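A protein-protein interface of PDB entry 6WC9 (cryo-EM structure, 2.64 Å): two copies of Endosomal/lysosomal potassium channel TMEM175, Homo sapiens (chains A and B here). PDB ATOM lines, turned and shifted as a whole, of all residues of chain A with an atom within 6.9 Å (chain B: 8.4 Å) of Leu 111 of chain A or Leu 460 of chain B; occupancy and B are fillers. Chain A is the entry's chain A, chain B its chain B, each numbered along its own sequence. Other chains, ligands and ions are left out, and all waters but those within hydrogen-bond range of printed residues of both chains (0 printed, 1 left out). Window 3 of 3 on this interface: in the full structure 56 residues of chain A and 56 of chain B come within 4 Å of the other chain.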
ATOM      1  N   MET A  36       5.301 -20.050  -9.980  1.00  0.00           N
ATOM      2  CA  MET A  36       4.522 -19.004 -10.630  1.00  0.00           C
ATOM      3  C   MET A  36       3.893 -19.514 -11.920  1.00  0.00           C
ATOM      4  O   MET A  36       2.712 -19.261 -12.191  1.00  0.00           O
ATOM      5  CB  MET A  36       5.415 -17.794 -10.899  1.00  0.00           C
ATOM      6  CG  MET A  36       4.672 -16.531 -11.286  1.00  0.00           C
ATOM      7  SD  MET A  36       5.780 -15.180 -11.713  1.00  0.00           S
ATOM      8  CE  MET A  36       6.444 -15.766 -13.261  1.00  0.00           C
ATOM      9  N   THR A 105      12.188 -15.090 -12.298  1.00  0.00           N
ATOM     10  CA  THR A 105      11.186 -14.101 -11.950  1.00  0.00           C
ATOM     11  C   THR A 105      11.582 -13.370 -10.671  1.00  0.00           C
ATOM     12  O   THR A 105      12.621 -13.634 -10.061  1.00  0.00           O
ATOM     13  CB  THR A 105       9.815 -14.762 -11.793  1.00  0.00           C
ATOM     14  OG1 THR A 105       8.791 -13.762 -11.831  1.00  0.00           O
ATOM     15  CG2 THR A 105       9.718 -15.508 -10.479  1.00  0.00           C
ATOM     16  N   ASP A 106      10.734 -12.434 -10.268  1.00  0.00           N
ATOM     17  CA  ASP A 106      10.903 -11.707  -9.019  1.00  0.00           C
ATOM     18  C   ASP A 106       9.541 -11.149  -8.619  1.00  0.00           C
ATOM     19  O   ASP A 106       8.515 -11.487  -9.216  1.00  0.00           O
ATOM     20  CB  ASP A 106      11.972 -10.619  -9.158  1.00  0.00           C
ATOM     21  CG  ASP A 106      11.643  -9.606 -10.230  1.00  0.00           C
ATOM     22  OD1 ASP A 106      10.644  -9.798 -10.950  1.00  0.00           O
ATOM     23  OD2 ASP A 106      12.386  -8.612 -10.351  1.00  0.00           O
ATOM     24  N   ASP A 107       9.534 -10.292  -7.599  1.00  0.00           N
ATOM     25  CA  ASP A 107       8.276  -9.782  -7.065  1.00  0.00           C
ATOM     26  C   ASP A 107       7.508  -8.988  -8.115  1.00  0.00           C
ATOM     27  O   ASP A 107       6.312  -9.217  -8.337  1.00  0.00           O
ATOM     28  CB  ASP A 107       8.559  -8.922  -5.835  1.00  0.00           C
ATOM     29  CG  ASP A 107       9.210  -9.706  -4.713  1.00  0.00           C
ATOM     30  OD1 ASP A 107       8.953 -10.923  -4.609  1.00  0.00           O
ATOM     31  OD2 ASP A 107       9.977  -9.105  -3.932  1.00  0.00           O
ATOM     32  N   THR A 108       8.184  -8.044  -8.770  1.00  0.00           N
ATOM     33  CA  THR A 108       7.519  -7.218  -9.769  1.00  0.00           C
ATOM     34  C   THR A 108       6.992  -8.063 -10.921  1.00  0.00           C
ATOM     35  O   THR A 108       5.867  -7.854 -11.391  1.00  0.00           O
ATOM     36  CB  THR A 108       8.482  -6.147 -10.278  1.00  0.00           C
ATOM     37  OG1 THR A 108       8.815  -5.256  -9.206  1.00  0.00           O
ATOM     38  CG2 THR A 108       7.867  -5.354 -11.414  1.00  0.00           C
ATOM     39  N   LEU A 109       7.793  -9.018 -11.393  1.00  0.00           N
ATOM     40  CA  LEU A 109       7.343  -9.883 -12.476  1.00  0.00           C
ATOM     41  C   LEU A 109       6.158 -10.734 -12.043  1.00  0.00           C
ATOM     42  O   LEU A 109       5.240 -10.973 -12.831  1.00  0.00           O
ATOM     43  CB  LEU A 109       8.491 -10.767 -12.955  1.00  0.00           C
ATOM     44  CG  LEU A 109       9.471 -10.094 -13.908  1.00  0.00           C
ATOM     45  CD1 LEU A 109      10.698 -10.947 -14.102  1.00  0.00           C
ATOM     46  CD2 LEU A 109       8.802  -9.828 -15.228  1.00  0.00           C
ATOM     47  N   ALA A 110       6.157 -11.197 -10.793  1.00  0.00           N
ATOM     48  CA  ALA A 110       5.032 -11.982 -10.299  1.00  0.00           C
ATOM     49  C   ALA A 110       3.752 -11.154 -10.255  1.00  0.00           C
ATOM     50  O   ALA A 110       2.677 -11.633 -10.636  1.00  0.00           O
ATOM     51  CB  ALA A 110       5.361 -12.541  -8.918  1.00  0.00           C
ATOM     52  N   LEU A 111       3.848  -9.904  -9.802  1.00  0.00           N
ATOM     53  CA  LEU A 111       2.666  -9.049  -9.764  1.00  0.00           C
ATOM     54  C   LEU A 111       2.173  -8.722 -11.170  1.00  0.00           C
ATOM     55  O   LEU A 111       0.962  -8.718 -11.431  1.00  0.00           O
ATOM     56  CB  LEU A 111       2.982  -7.778  -8.978  1.00  0.00           C
ATOM     57  CG  LEU A 111       3.377  -8.035  -7.523  1.00  0.00           C
ATOM     58  CD1 LEU A 111       4.058  -6.831  -6.908  1.00  0.00           C
ATOM     59  CD2 LEU A 111       2.172  -8.422  -6.708  1.00  0.00           C
ATOM     60  N   LEU A 112       3.096  -8.459 -12.096  1.00  0.00           N
ATOM     61  CA  LEU A 112       2.701  -8.207 -13.476  1.00  0.00           C
ATOM     62  C   LEU A 112       2.072  -9.445 -14.106  1.00  0.00           C
ATOM     63  O   LEU A 112       1.149  -9.339 -14.920  1.00  0.00           O
ATOM     64  CB  LEU A 112       3.910  -7.742 -14.283  1.00  0.00           C
ATOM     65  CG  LEU A 112       4.317  -6.281 -14.109  1.00  0.00           C
ATOM     66  CD1 LEU A 112       5.687  -6.050 -14.696  1.00  0.00           C
ATOM     67  CD2 LEU A 112       3.302  -5.356 -14.748  1.00  0.00           C
ATOM     68  N   ASN A 113       2.554 -10.632 -13.736  1.00  0.00           N
ATOM     69  CA  ASN A 113       1.949 -11.866 -14.222  1.00  0.00           C
ATOM     70  C   ASN A 113       0.544 -12.045 -13.663  1.00  0.00           C
ATOM     71  O   ASN A 113      -0.349 -12.538 -14.360  1.00  0.00           O
ATOM     72  CB  ASN A 113       2.837 -13.052 -13.852  1.00  0.00           C
ATOM     73  CG  ASN A 113       2.398 -14.337 -14.512  1.00  0.00           C
ATOM     74  OD1 ASN A 113       2.632 -14.547 -15.698  1.00  0.00           O
ATOM     75  ND2 ASN A 113       1.767 -15.208 -13.743  1.00  0.00           N
ATOM     76  N   LEU A 114       0.334 -11.665 -12.403  1.00  0.00           N
ATOM     77  CA  LEU A 114      -1.020 -11.667 -11.857  1.00  0.00           C
ATOM     78  C   LEU A 114      -1.926 -10.735 -12.649  1.00  0.00           C
ATOM     79  O   LEU A 114      -3.083 -11.069 -12.935  1.00  0.00           O
ATOM     80  CB  LEU A 114      -0.990 -11.261 -10.387  1.00  0.00           C
ATOM     81  CG  LEU A 114      -0.476 -12.317  -9.414  1.00  0.00           C
ATOM     82  CD1 LEU A 114      -0.125 -11.672  -8.089  1.00  0.00           C
ATOM     83  CD2 LEU A 114      -1.502 -13.417  -9.227  1.00  0.00           C
ATOM     84  N   ALA A 115      -1.414  -9.559 -13.013  1.00  0.00           N
ATOM     85  CA  ALA A 115      -2.187  -8.643 -13.846  1.00  0.00           C
ATOM     86  C   ALA A 115      -2.520  -9.267 -15.196  1.00  0.00           C
ATOM     87  O   ALA A 115      -3.642  -9.126 -15.699  1.00  0.00           O
ATOM     88  CB  ALA A 115      -1.421  -7.337 -14.034  1.00  0.00           C
ATOM     89  N   CYS A 116      -1.551  -9.951 -15.805  1.00  0.00           N
ATOM     90  CA  CYS A 116      -1.791 -10.606 -17.087  1.00  0.00           C
ATOM     91  C   CYS A 116      -2.860 -11.685 -16.968  1.00  0.00           C
ATOM     92  O   CYS A 116      -3.729 -11.812 -17.840  1.00  0.00           O
ATOM     93  CB  CYS A 116      -0.489 -11.206 -17.616  1.00  0.00           C
ATOM     94  SG  CYS A 116      -0.602 -11.877 -19.283  1.00  0.00           S
ATOM     95  N   VAL A 153       0.545  -5.771 -21.017  1.00  0.00           N
ATOM     96  CA  VAL A 153       1.156  -6.347 -19.822  1.00  0.00           C
ATOM     97  C   VAL A 153       2.348  -7.212 -20.206  1.00  0.00           C
ATOM     98  O   VAL A 153       3.393  -7.191 -19.540  1.00  0.00           O
ATOM     99  CB  VAL A 153       0.111  -7.138 -19.017  1.00  0.00           C
ATOM    100  CG1 VAL A 153       0.767  -7.841 -17.847  1.00  0.00           C
ATOM    101  CG2 VAL A 153      -0.983  -6.212 -18.526  1.00  0.00           C
ATOM    102  N   PHE B 317     -10.030 -11.282  -6.708  1.00  0.00           N
ATOM    103  CA  PHE B 317      -8.850 -11.734  -7.429  1.00  0.00           C
ATOM    104  C   PHE B 317      -7.599 -11.054  -6.897  1.00  0.00           C
ATOM    105  O   PHE B 317      -6.583 -11.710  -6.660  1.00  0.00           O
ATOM    106  CB  PHE B 317      -9.017 -11.471  -8.924  1.00  0.00           C
ATOM    107  CG  PHE B 317      -7.960 -12.111  -9.769  1.00  0.00           C
ATOM    108  CD1 PHE B 317      -8.172 -13.347 -10.345  1.00  0.00           C
ATOM    109  CD2 PHE B 317      -6.750 -11.481  -9.984  1.00  0.00           C
ATOM    110  CE1 PHE B 317      -7.205 -13.935 -11.115  1.00  0.00           C
ATOM    111  CE2 PHE B 317      -5.782 -12.069 -10.754  1.00  0.00           C
ATOM    112  CZ  PHE B 317      -6.008 -13.297 -11.320  1.00  0.00           C
ATOM    113  N   ALA B 318      -7.655  -9.737  -6.696  1.00  0.00           N
ATOM    114  CA  ALA B 318      -6.491  -9.029  -6.176  1.00  0.00           C
ATOM    115  C   ALA B 318      -6.085  -9.567  -4.810  1.00  0.00           C
ATOM    116  O   ALA B 318      -4.905  -9.847  -4.565  1.00  0.00           O
ATOM    117  CB  ALA B 318      -6.782  -7.533  -6.101  1.00  0.00           C
ATOM    118  N   GLY B 321      -4.753 -13.154  -5.017  1.00  0.00           N
ATOM    119  CA  GLY B 321      -3.466 -13.174  -5.684  1.00  0.00           C
ATOM    120  C   GLY B 321      -2.350 -12.632  -4.819  1.00  0.00           C
ATOM    121  O   GLY B 321      -1.228 -13.132  -4.863  1.00  0.00           O
ATOM    122  N   LEU B 322      -2.640 -11.614  -4.011  1.00  0.00           N
ATOM    123  CA  LEU B 322      -1.616 -11.099  -3.110  1.00  0.00           C
ATOM    124  C   LEU B 322      -1.357 -12.056  -1.955  1.00  0.00           C
ATOM    125  O   LEU B 322      -0.216 -12.177  -1.493  1.00  0.00           O
ATOM    126  CB  LEU B 322      -2.023  -9.722  -2.600  1.00  0.00           C
ATOM    127  CG  LEU B 322      -2.092  -8.650  -3.687  1.00  0.00           C
ATOM    128  CD1 LEU B 322      -2.675  -7.365  -3.141  1.00  0.00           C
ATOM    129  CD2 LEU B 322      -0.726  -8.399  -4.284  1.00  0.00           C
ATOM    130  N   LEU B 323      -2.386 -12.761  -1.489  1.00  0.00           N
ATOM    131  CA  LEU B 323      -2.154 -13.795  -0.487  1.00  0.00           C
ATOM    132  C   LEU B 323      -1.338 -14.948  -1.064  1.00  0.00           C
ATOM    133  O   LEU B 323      -0.461 -15.494  -0.385  1.00  0.00           O
ATOM    134  CB  LEU B 323      -3.485 -14.289   0.070  1.00  0.00           C
ATOM    135  CG  LEU B 323      -4.169 -13.355   1.069  1.00  0.00           C
ATOM    136  CD1 LEU B 323      -5.547 -13.858   1.392  1.00  0.00           C
ATOM    137  CD2 LEU B 323      -3.363 -13.196   2.342  1.00  0.00           C
ATOM    138  N   TRP B 324      -1.605 -15.328  -2.317  1.00  0.00           N
ATOM    139  CA  TRP B 324      -0.764 -16.316  -2.982  1.00  0.00           C
ATOM    140  C   TRP B 324       0.657 -15.801  -3.152  1.00  0.00           C
ATOM    141  O   TRP B 324       1.617 -16.564  -3.042  1.00  0.00           O
ATOM    142  CB  TRP B 324      -1.353 -16.702  -4.342  1.00  0.00           C
ATOM    143  CG  TRP B 324      -0.423 -17.566  -5.127  1.00  0.00           C
ATOM    144  CD1 TRP B 324      -0.347 -18.922  -5.095  1.00  0.00           C
ATOM    145  CD2 TRP B 324       0.590 -17.129  -6.039  1.00  0.00           C
ATOM    146  NE1 TRP B 324       0.645 -19.359  -5.929  1.00  0.00           N
ATOM    147  CE2 TRP B 324       1.236 -18.277  -6.520  1.00  0.00           C
ATOM    148  CE3 TRP B 324       1.013 -15.879  -6.491  1.00  0.00           C
ATOM    149  CZ2 TRP B 324       2.277 -18.214  -7.435  1.00  0.00           C
ATOM    150  CZ3 TRP B 324       2.043 -15.819  -7.394  1.00  0.00           C
ATOM    151  CH2 TRP B 324       2.665 -16.978  -7.860  1.00  0.00           C
ATOM    152  N   PHE B 325       0.807 -14.512  -3.451  1.00  0.00           N
ATOM    153  CA  PHE B 325       2.126 -13.901  -3.556  1.00  0.00           C
ATOM    154  C   PHE B 325       2.895 -14.034  -2.247  1.00  0.00           C
ATOM    155  O   PHE B 325       4.078 -14.397  -2.239  1.00  0.00           O
ATOM    156  CB  PHE B 325       1.957 -12.435  -3.960  1.00  0.00           C
ATOM    157  CG  PHE B 325       3.233 -11.657  -4.023  1.00  0.00           C
ATOM    158  CD1 PHE B 325       4.110 -11.825  -5.074  1.00  0.00           C
ATOM    159  CD2 PHE B 325       3.543 -10.735  -3.042  1.00  0.00           C
ATOM    160  CE1 PHE B 325       5.277 -11.104  -5.135  1.00  0.00           C
ATOM    161  CE2 PHE B 325       4.707 -10.013  -3.100  1.00  0.00           C
ATOM    162  CZ  PHE B 325       5.574 -10.196  -4.147  1.00  0.00           C
ATOM    163  N   ALA B 326       2.230 -13.751  -1.128  1.00  0.00           N
ATOM    164  CA  ALA B 326       2.865 -13.909   0.177  1.00  0.00           C
ATOM    165  C   ALA B 326       3.237 -15.364   0.441  1.00  0.00           C
ATOM    166  O   ALA B 326       4.353 -15.662   0.881  1.00  0.00           O
ATOM    167  CB  ALA B 326       1.938 -13.384   1.270  1.00  0.00           C
ATOM    168  N   HIS B 328       3.819 -17.709  -1.698  1.00  0.00           N
ATOM    169  CA  HIS B 328       4.878 -18.092  -2.621  1.00  0.00           C
ATOM    170  C   HIS B 328       6.225 -17.546  -2.170  1.00  0.00           C
ATOM    171  O   HIS B 328       7.227 -18.274  -2.160  1.00  0.00           O
ATOM    172  CB  HIS B 328       4.484 -17.593  -4.015  1.00  0.00           C
ATOM    173  CG  HIS B 328       5.596 -17.573  -5.015  1.00  0.00           C
ATOM    174  ND1 HIS B 328       6.224 -16.408  -5.400  1.00  0.00           N
ATOM    175  CD2 HIS B 328       6.152 -18.561  -5.754  1.00  0.00           C
ATOM    176  CE1 HIS B 328       7.141 -16.686  -6.308  1.00  0.00           C
ATOM    177  NE2 HIS B 328       7.117 -17.985  -6.540  1.00  0.00           N
ATOM    178  N   SER B 329       6.263 -16.278  -1.761  1.00  0.00           N
ATOM    179  CA  SER B 329       7.495 -15.707  -1.237  1.00  0.00           C
ATOM    180  C   SER B 329       7.961 -16.452   0.006  1.00  0.00           C
ATOM    181  O   SER B 329       9.159 -16.702   0.176  1.00  0.00           O
ATOM    182  CB  SER B 329       7.288 -14.227  -0.927  1.00  0.00           C
ATOM    183  OG  SER B 329       6.641 -13.567  -1.996  1.00  0.00           O
ATOM    184  N   LYS B 422       5.966  -8.479   4.357  1.00  0.00           N
ATOM    185  CA  LYS B 422       5.121  -9.094   3.342  1.00  0.00           C
ATOM    186  C   LYS B 422       4.024  -9.944   3.961  1.00  0.00           C
ATOM    187  O   LYS B 422       2.918 -10.022   3.415  1.00  0.00           O
ATOM    188  CB  LYS B 422       5.982  -9.935   2.403  1.00  0.00           C
ATOM    189  CG  LYS B 422       5.513  -9.957   0.965  1.00  0.00           C
ATOM    190  CD  LYS B 422       6.451 -10.761   0.088  1.00  0.00           C
ATOM    191  CE  LYS B 422       7.773 -10.050  -0.113  1.00  0.00           C
ATOM    192  NZ  LYS B 422       8.660 -10.770  -1.054  1.00  0.00           N
ATOM    193  N   LEU B 425       1.521  -7.487   6.392  1.00  0.00           N
ATOM    194  CA  LEU B 425       0.840  -6.369   5.752  1.00  0.00           C
ATOM    195  C   LEU B 425      -0.676  -6.525   5.817  1.00  0.00           C
ATOM    196  O   LEU B 425      -1.384  -5.646   6.317  1.00  0.00           O
ATOM    197  CB  LEU B 425       1.316  -6.252   4.306  1.00  0.00           C
ATOM    198  CG  LEU B 425       0.825  -5.059   3.491  1.00  0.00           C
ATOM    199  CD1 LEU B 425       1.013  -3.762   4.247  1.00  0.00           C
ATOM    200  CD2 LEU B 425       1.563  -5.019   2.177  1.00  0.00           C
ATOM    201  N   ALA B 454      -4.680   0.178  -1.938  1.00  0.00           N
ATOM    202  CA  ALA B 454      -3.335   0.534  -1.510  1.00  0.00           C
ATOM    203  C   ALA B 454      -2.457  -0.677  -1.216  1.00  0.00           C
ATOM    204  O   ALA B 454      -1.273  -0.679  -1.566  1.00  0.00           O
ATOM    205  CB  ALA B 454      -3.415   1.431  -0.272  1.00  0.00           C
ATOM    206  N   VAL B 455      -3.005  -1.699  -0.564  1.00  0.00           N
ATOM    207  CA  VAL B 455      -2.225  -2.879  -0.194  1.00  0.00           C
ATOM    208  C   VAL B 455      -1.455  -3.393  -1.407  1.00  0.00           C
ATOM    209  O   VAL B 455      -0.280  -3.765  -1.275  1.00  0.00           O
ATOM    210  CB  VAL B 455      -3.125  -3.972   0.405  1.00  0.00           C
ATOM    211  CG1 VAL B 455      -2.360  -5.273   0.560  1.00  0.00           C
ATOM    212  CG2 VAL B 455      -3.664  -3.526   1.745  1.00  0.00           C
ATOM    213  N   PRO B 456      -2.058  -3.437  -2.599  1.00  0.00           N
ATOM    214  CA  PRO B 456      -1.269  -3.823  -3.784  1.00  0.00           C
ATOM    215  C   PRO B 456      -0.095  -2.896  -4.046  1.00  0.00           C
ATOM    216  O   PRO B 456       1.020  -3.365  -4.308  1.00  0.00           O
ATOM    217  CB  PRO B 456      -2.304  -3.779  -4.916  1.00  0.00           C
ATOM    218  CG  PRO B 456      -3.612  -3.929  -4.253  1.00  0.00           C
ATOM    219  CD  PRO B 456      -3.487  -3.296  -2.914  1.00  0.00           C
ATOM    220  N   CYS B 457      -0.319  -1.581  -3.990  1.00  0.00           N
ATOM    221  CA  CYS B 457       0.772  -0.638  -4.202  1.00  0.00           C
ATOM    222  C   CYS B 457       1.838  -0.770  -3.125  1.00  0.00           C
ATOM    223  O   CYS B 457       3.018  -0.505  -3.382  1.00  0.00           O
ATOM    224  CB  CYS B 457       0.226   0.789  -4.242  1.00  0.00           C
ATOM    225  SG  CYS B 457      -1.013   1.070  -5.524  1.00  0.00           S
ATOM    226  N   ALA B 458       1.446  -1.169  -1.916  1.00  0.00           N
ATOM    227  CA  ALA B 458       2.426  -1.431  -0.868  1.00  0.00           C
ATOM    228  C   ALA B 458       3.259  -2.661  -1.201  1.00  0.00           C
ATOM    229  O   ALA B 458       4.483  -2.660  -1.033  1.00  0.00           O
ATOM    230  CB  ALA B 458       1.719  -1.602   0.474  1.00  0.00           C
ATOM    231  N   PHE B 459       2.607  -3.727  -1.673  1.00  0.00           N
ATOM    232  CA  PHE B 459       3.346  -4.906  -2.110  1.00  0.00           C
ATOM    233  C   PHE B 459       4.321  -4.557  -3.227  1.00  0.00           C
ATOM    234  O   PHE B 459       5.439  -5.083  -3.274  1.00  0.00           O
ATOM    235  CB  PHE B 459       2.377  -5.990  -2.574  1.00  0.00           C
ATOM    236  CG  PHE B 459       1.858  -6.859  -1.468  1.00  0.00           C
ATOM    237  CD1 PHE B 459       2.668  -7.812  -0.882  1.00  0.00           C
ATOM    238  CD2 PHE B 459       0.557  -6.731  -1.021  1.00  0.00           C
ATOM    239  CE1 PHE B 459       2.192  -8.614   0.130  1.00  0.00           C
ATOM    240  CE2 PHE B 459       0.079  -7.531  -0.008  1.00  0.00           C
ATOM    241  CZ  PHE B 459       0.897  -8.473   0.566  1.00  0.00           C
ATOM    242  N   LEU B 460       3.913  -3.672  -4.135  1.00  0.00           N
ATOM    243  CA  LEU B 460       4.763  -3.326  -5.269  1.00  0.00           C
ATOM    244  C   LEU B 460       5.967  -2.500  -4.833  1.00  0.00           C
ATOM    245  O   LEU B 460       7.073  -2.685  -5.352  1.00  0.00           O
ATOM    246  CB  LEU B 460       3.944  -2.573  -6.314  1.00  0.00           C
ATOM    247  CG  LEU B 460       4.384  -2.689  -7.774  1.00  0.00           C
ATOM    248  CD1 LEU B 460       3.210  -2.409  -8.690  1.00  0.00           C
ATOM    249  CD2 LEU B 460       5.527  -1.746  -8.078  1.00  0.00           C
ATOM    250  N   LEU B 461       5.774  -1.586  -3.883  1.00  0.00           N
ATOM    251  CA  LEU B 461       6.836  -0.721  -3.387  1.00  0.00           C
ATOM    252  C   LEU B 461       7.301  -1.128  -1.993  1.00  0.00           C
ATOM    253  O   LEU B 461       7.794  -0.296  -1.231  1.00  0.00           O
ATOM    254  CB  LEU B 461       6.374   0.734  -3.372  1.00  0.00           C
ATOM    255  CG  LEU B 461       5.691   1.268  -4.626  1.00  0.00           C
ATOM    256  CD1 LEU B 461       4.922   2.525  -4.283  1.00  0.00           C
ATOM    257  CD2 LEU B 461       6.711   1.535  -5.709  1.00  0.00           C
ATOM    258  N   LEU B 462       7.158  -2.408  -1.651  1.00  0.00           N
ATOM    259  CA  LEU B 462       7.421  -2.834  -0.282  1.00  0.00           C
ATOM    260  C   LEU B 462       8.882  -2.636   0.098  1.00  0.00           C
ATOM    261  O   LEU B 462       9.185  -2.295   1.244  1.00  0.00           O
ATOM    262  CB  LEU B 462       7.014  -4.293  -0.105  1.00  0.00           C
ATOM    263  CG  LEU B 462       6.856  -4.782   1.334  1.00  0.00           C
ATOM    264  CD1 LEU B 462       5.826  -3.958   2.092  1.00  0.00           C
ATOM    265  CD2 LEU B 462       6.467  -6.239   1.335  1.00  0.00           C
ATOM    266  N   ARG B 463       9.804  -2.848  -0.841  1.00  0.00           N
ATOM    267  CA  ARG B 463      11.220  -2.693  -0.521  1.00  0.00           C
ATOM    268  C   ARG B 463      11.566  -1.239  -0.219  1.00  0.00           C
ATOM    269  O   ARG B 463      12.283  -0.952   0.749  1.00  0.00           O
ATOM    270  CB  ARG B 463      12.070  -3.229  -1.670  1.00  0.00           C
ATOM    271  CG  ARG B 463      12.081  -4.743  -1.751  1.00  0.00           C
ATOM    272  CD  ARG B 463      12.702  -5.254  -3.034  1.00  0.00           C
ATOM    273  NE  ARG B 463      12.584  -6.706  -3.144  1.00  0.00           N
ATOM    274  CZ  ARG B 463      13.379  -7.571  -2.523  1.00  0.00           C
ATOM    275  NH1 ARG B 463      14.362  -7.137  -1.747  1.00  0.00           N
ATOM    276  NH2 ARG B 463      13.195  -8.875  -2.679  1.00  0.00           N
ATOM    277  N   LEU B 464      11.064  -0.310  -1.032  1.00  0.00           N
ATOM    278  CA  LEU B 464      11.311   1.106  -0.783  1.00  0.00           C
ATOM    279  C   LEU B 464      10.754   1.526   0.571  1.00  0.00           C
ATOM    280  O   LEU B 464      11.419   2.230   1.341  1.00  0.00           O
ATOM    281  CB  LEU B 464      10.693   1.947  -1.901  1.00  0.00           C
ATOM    282  CG  LEU B 464      11.474   2.053  -3.213  1.00  0.00           C
ATOM    283  CD1 LEU B 464      12.714   2.912  -3.032  1.00  0.00           C
ATOM    284  CD2 LEU B 464      11.848   0.677  -3.747  1.00  0.00           C
ATOM    285  N   LEU B 465       9.525   1.106   0.877  1.00  0.00           N
ATOM    286  CA  LEU B 465       8.913   1.475   2.147  1.00  0.00           C
ATOM    287  C   LEU B 465       9.661   0.854   3.319  1.00  0.00           C
ATOM    288  O   LEU B 465       9.818   1.484   4.369  1.00  0.00           O
ATOM    289  CB  LEU B 465       7.446   1.048   2.164  1.00  0.00           C
ATOM    290  CG  LEU B 465       6.573   1.616   1.046  1.00  0.00           C
ATOM    291  CD1 LEU B 465       5.258   0.856   0.971  1.00  0.00           C
ATOM    292  CD2 LEU B 465       6.333   3.098   1.253  1.00  0.00           C
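Hydrophobic or aromatic side chains of chain B within 4 Å of the printed part of chain A: Phe 317, Leu 322, Trp 324 and Phe 325.
Printed residues of chain A that touch a printed residue of chain B: Met 36, Asp 107, Leu 111 and Leu 114.
Hydrophobic or aromatic side chains of chain A within 4 Å of the printed part of chain B: Met 36, Leu 111 and Leu 114.
Among the printed residues, Asp or Glu carboxylates within 4 Å of a Lys or Arg side-chain nitrogen of the other chain: Asp 107 of chain A with Lys 422 of chain B and Asp 107 of chain A with Arg 463 of chain B.
CH2 of Trp 324 of chain B touches CA of Met 36 of chain A, 3.9 Å away.
Asp 107 of chain A touches Phe 325 of chain B (OD1 to CZ, 3.5 Å).
Leu 111 of chain A touches Leu 322 of chain B (CD2 to CD2, 3.8 Å).
Leu 111 of chain A touches Leu 460 of chain B (CD1 to CA, 3.9 Å).
O of Leu 114 of chain A touches CE2 of Phe 317 of chain B, at 3.6 Å.
Leu 114 of chain A touches Gly 321 of chain B (CD1 to O, 3.7 Å).
The side-chain hydroxyl (OG) of Ser 329 of chain B sits at hydrogen-bond distance from the backbone carbonyl oxygen (O) of Phe 325 of chain B (2.7 Å).
OG1 of Thr 105 of chain A sits at hydrogen-bond distance from SD of Met 36 of chain A, at 3.3 Å.
No position is printed for both chains.
Of the 8 pairs that touch across the chains among the printed residues, none has its exchanged pair printed and touching as well.
Leu 111 of chain A touches just these residues of chain B: Leu 322 (3.8 Å) and Leu 460 (3.9 Å).
Leu 460 of chain B touches just one residue of chain A: Leu 111.
Ala 110 of chain A touches none of the printed residues of chain B.
Of the printed residues of chain A, Trp 324 of chain B touches Met 36 (3.9 Å).
Printed residues of chain A within 4 Å of Leu 322 of chain B: Leu 111.
The nearest printed residue of chain B that does not touch Leu 111 of chain A is Phe 325 of chain B (4.2 Å).
NZ of Lys 422 of chain B is in salt-bridge range of OD1 of Asp 107 of chain A (3.6 Å).
The side-chain carboxylate of Asp 107 of chain A is in salt-bridge range of the guanidinium group of Arg 463 of chain B (3.5 Å).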
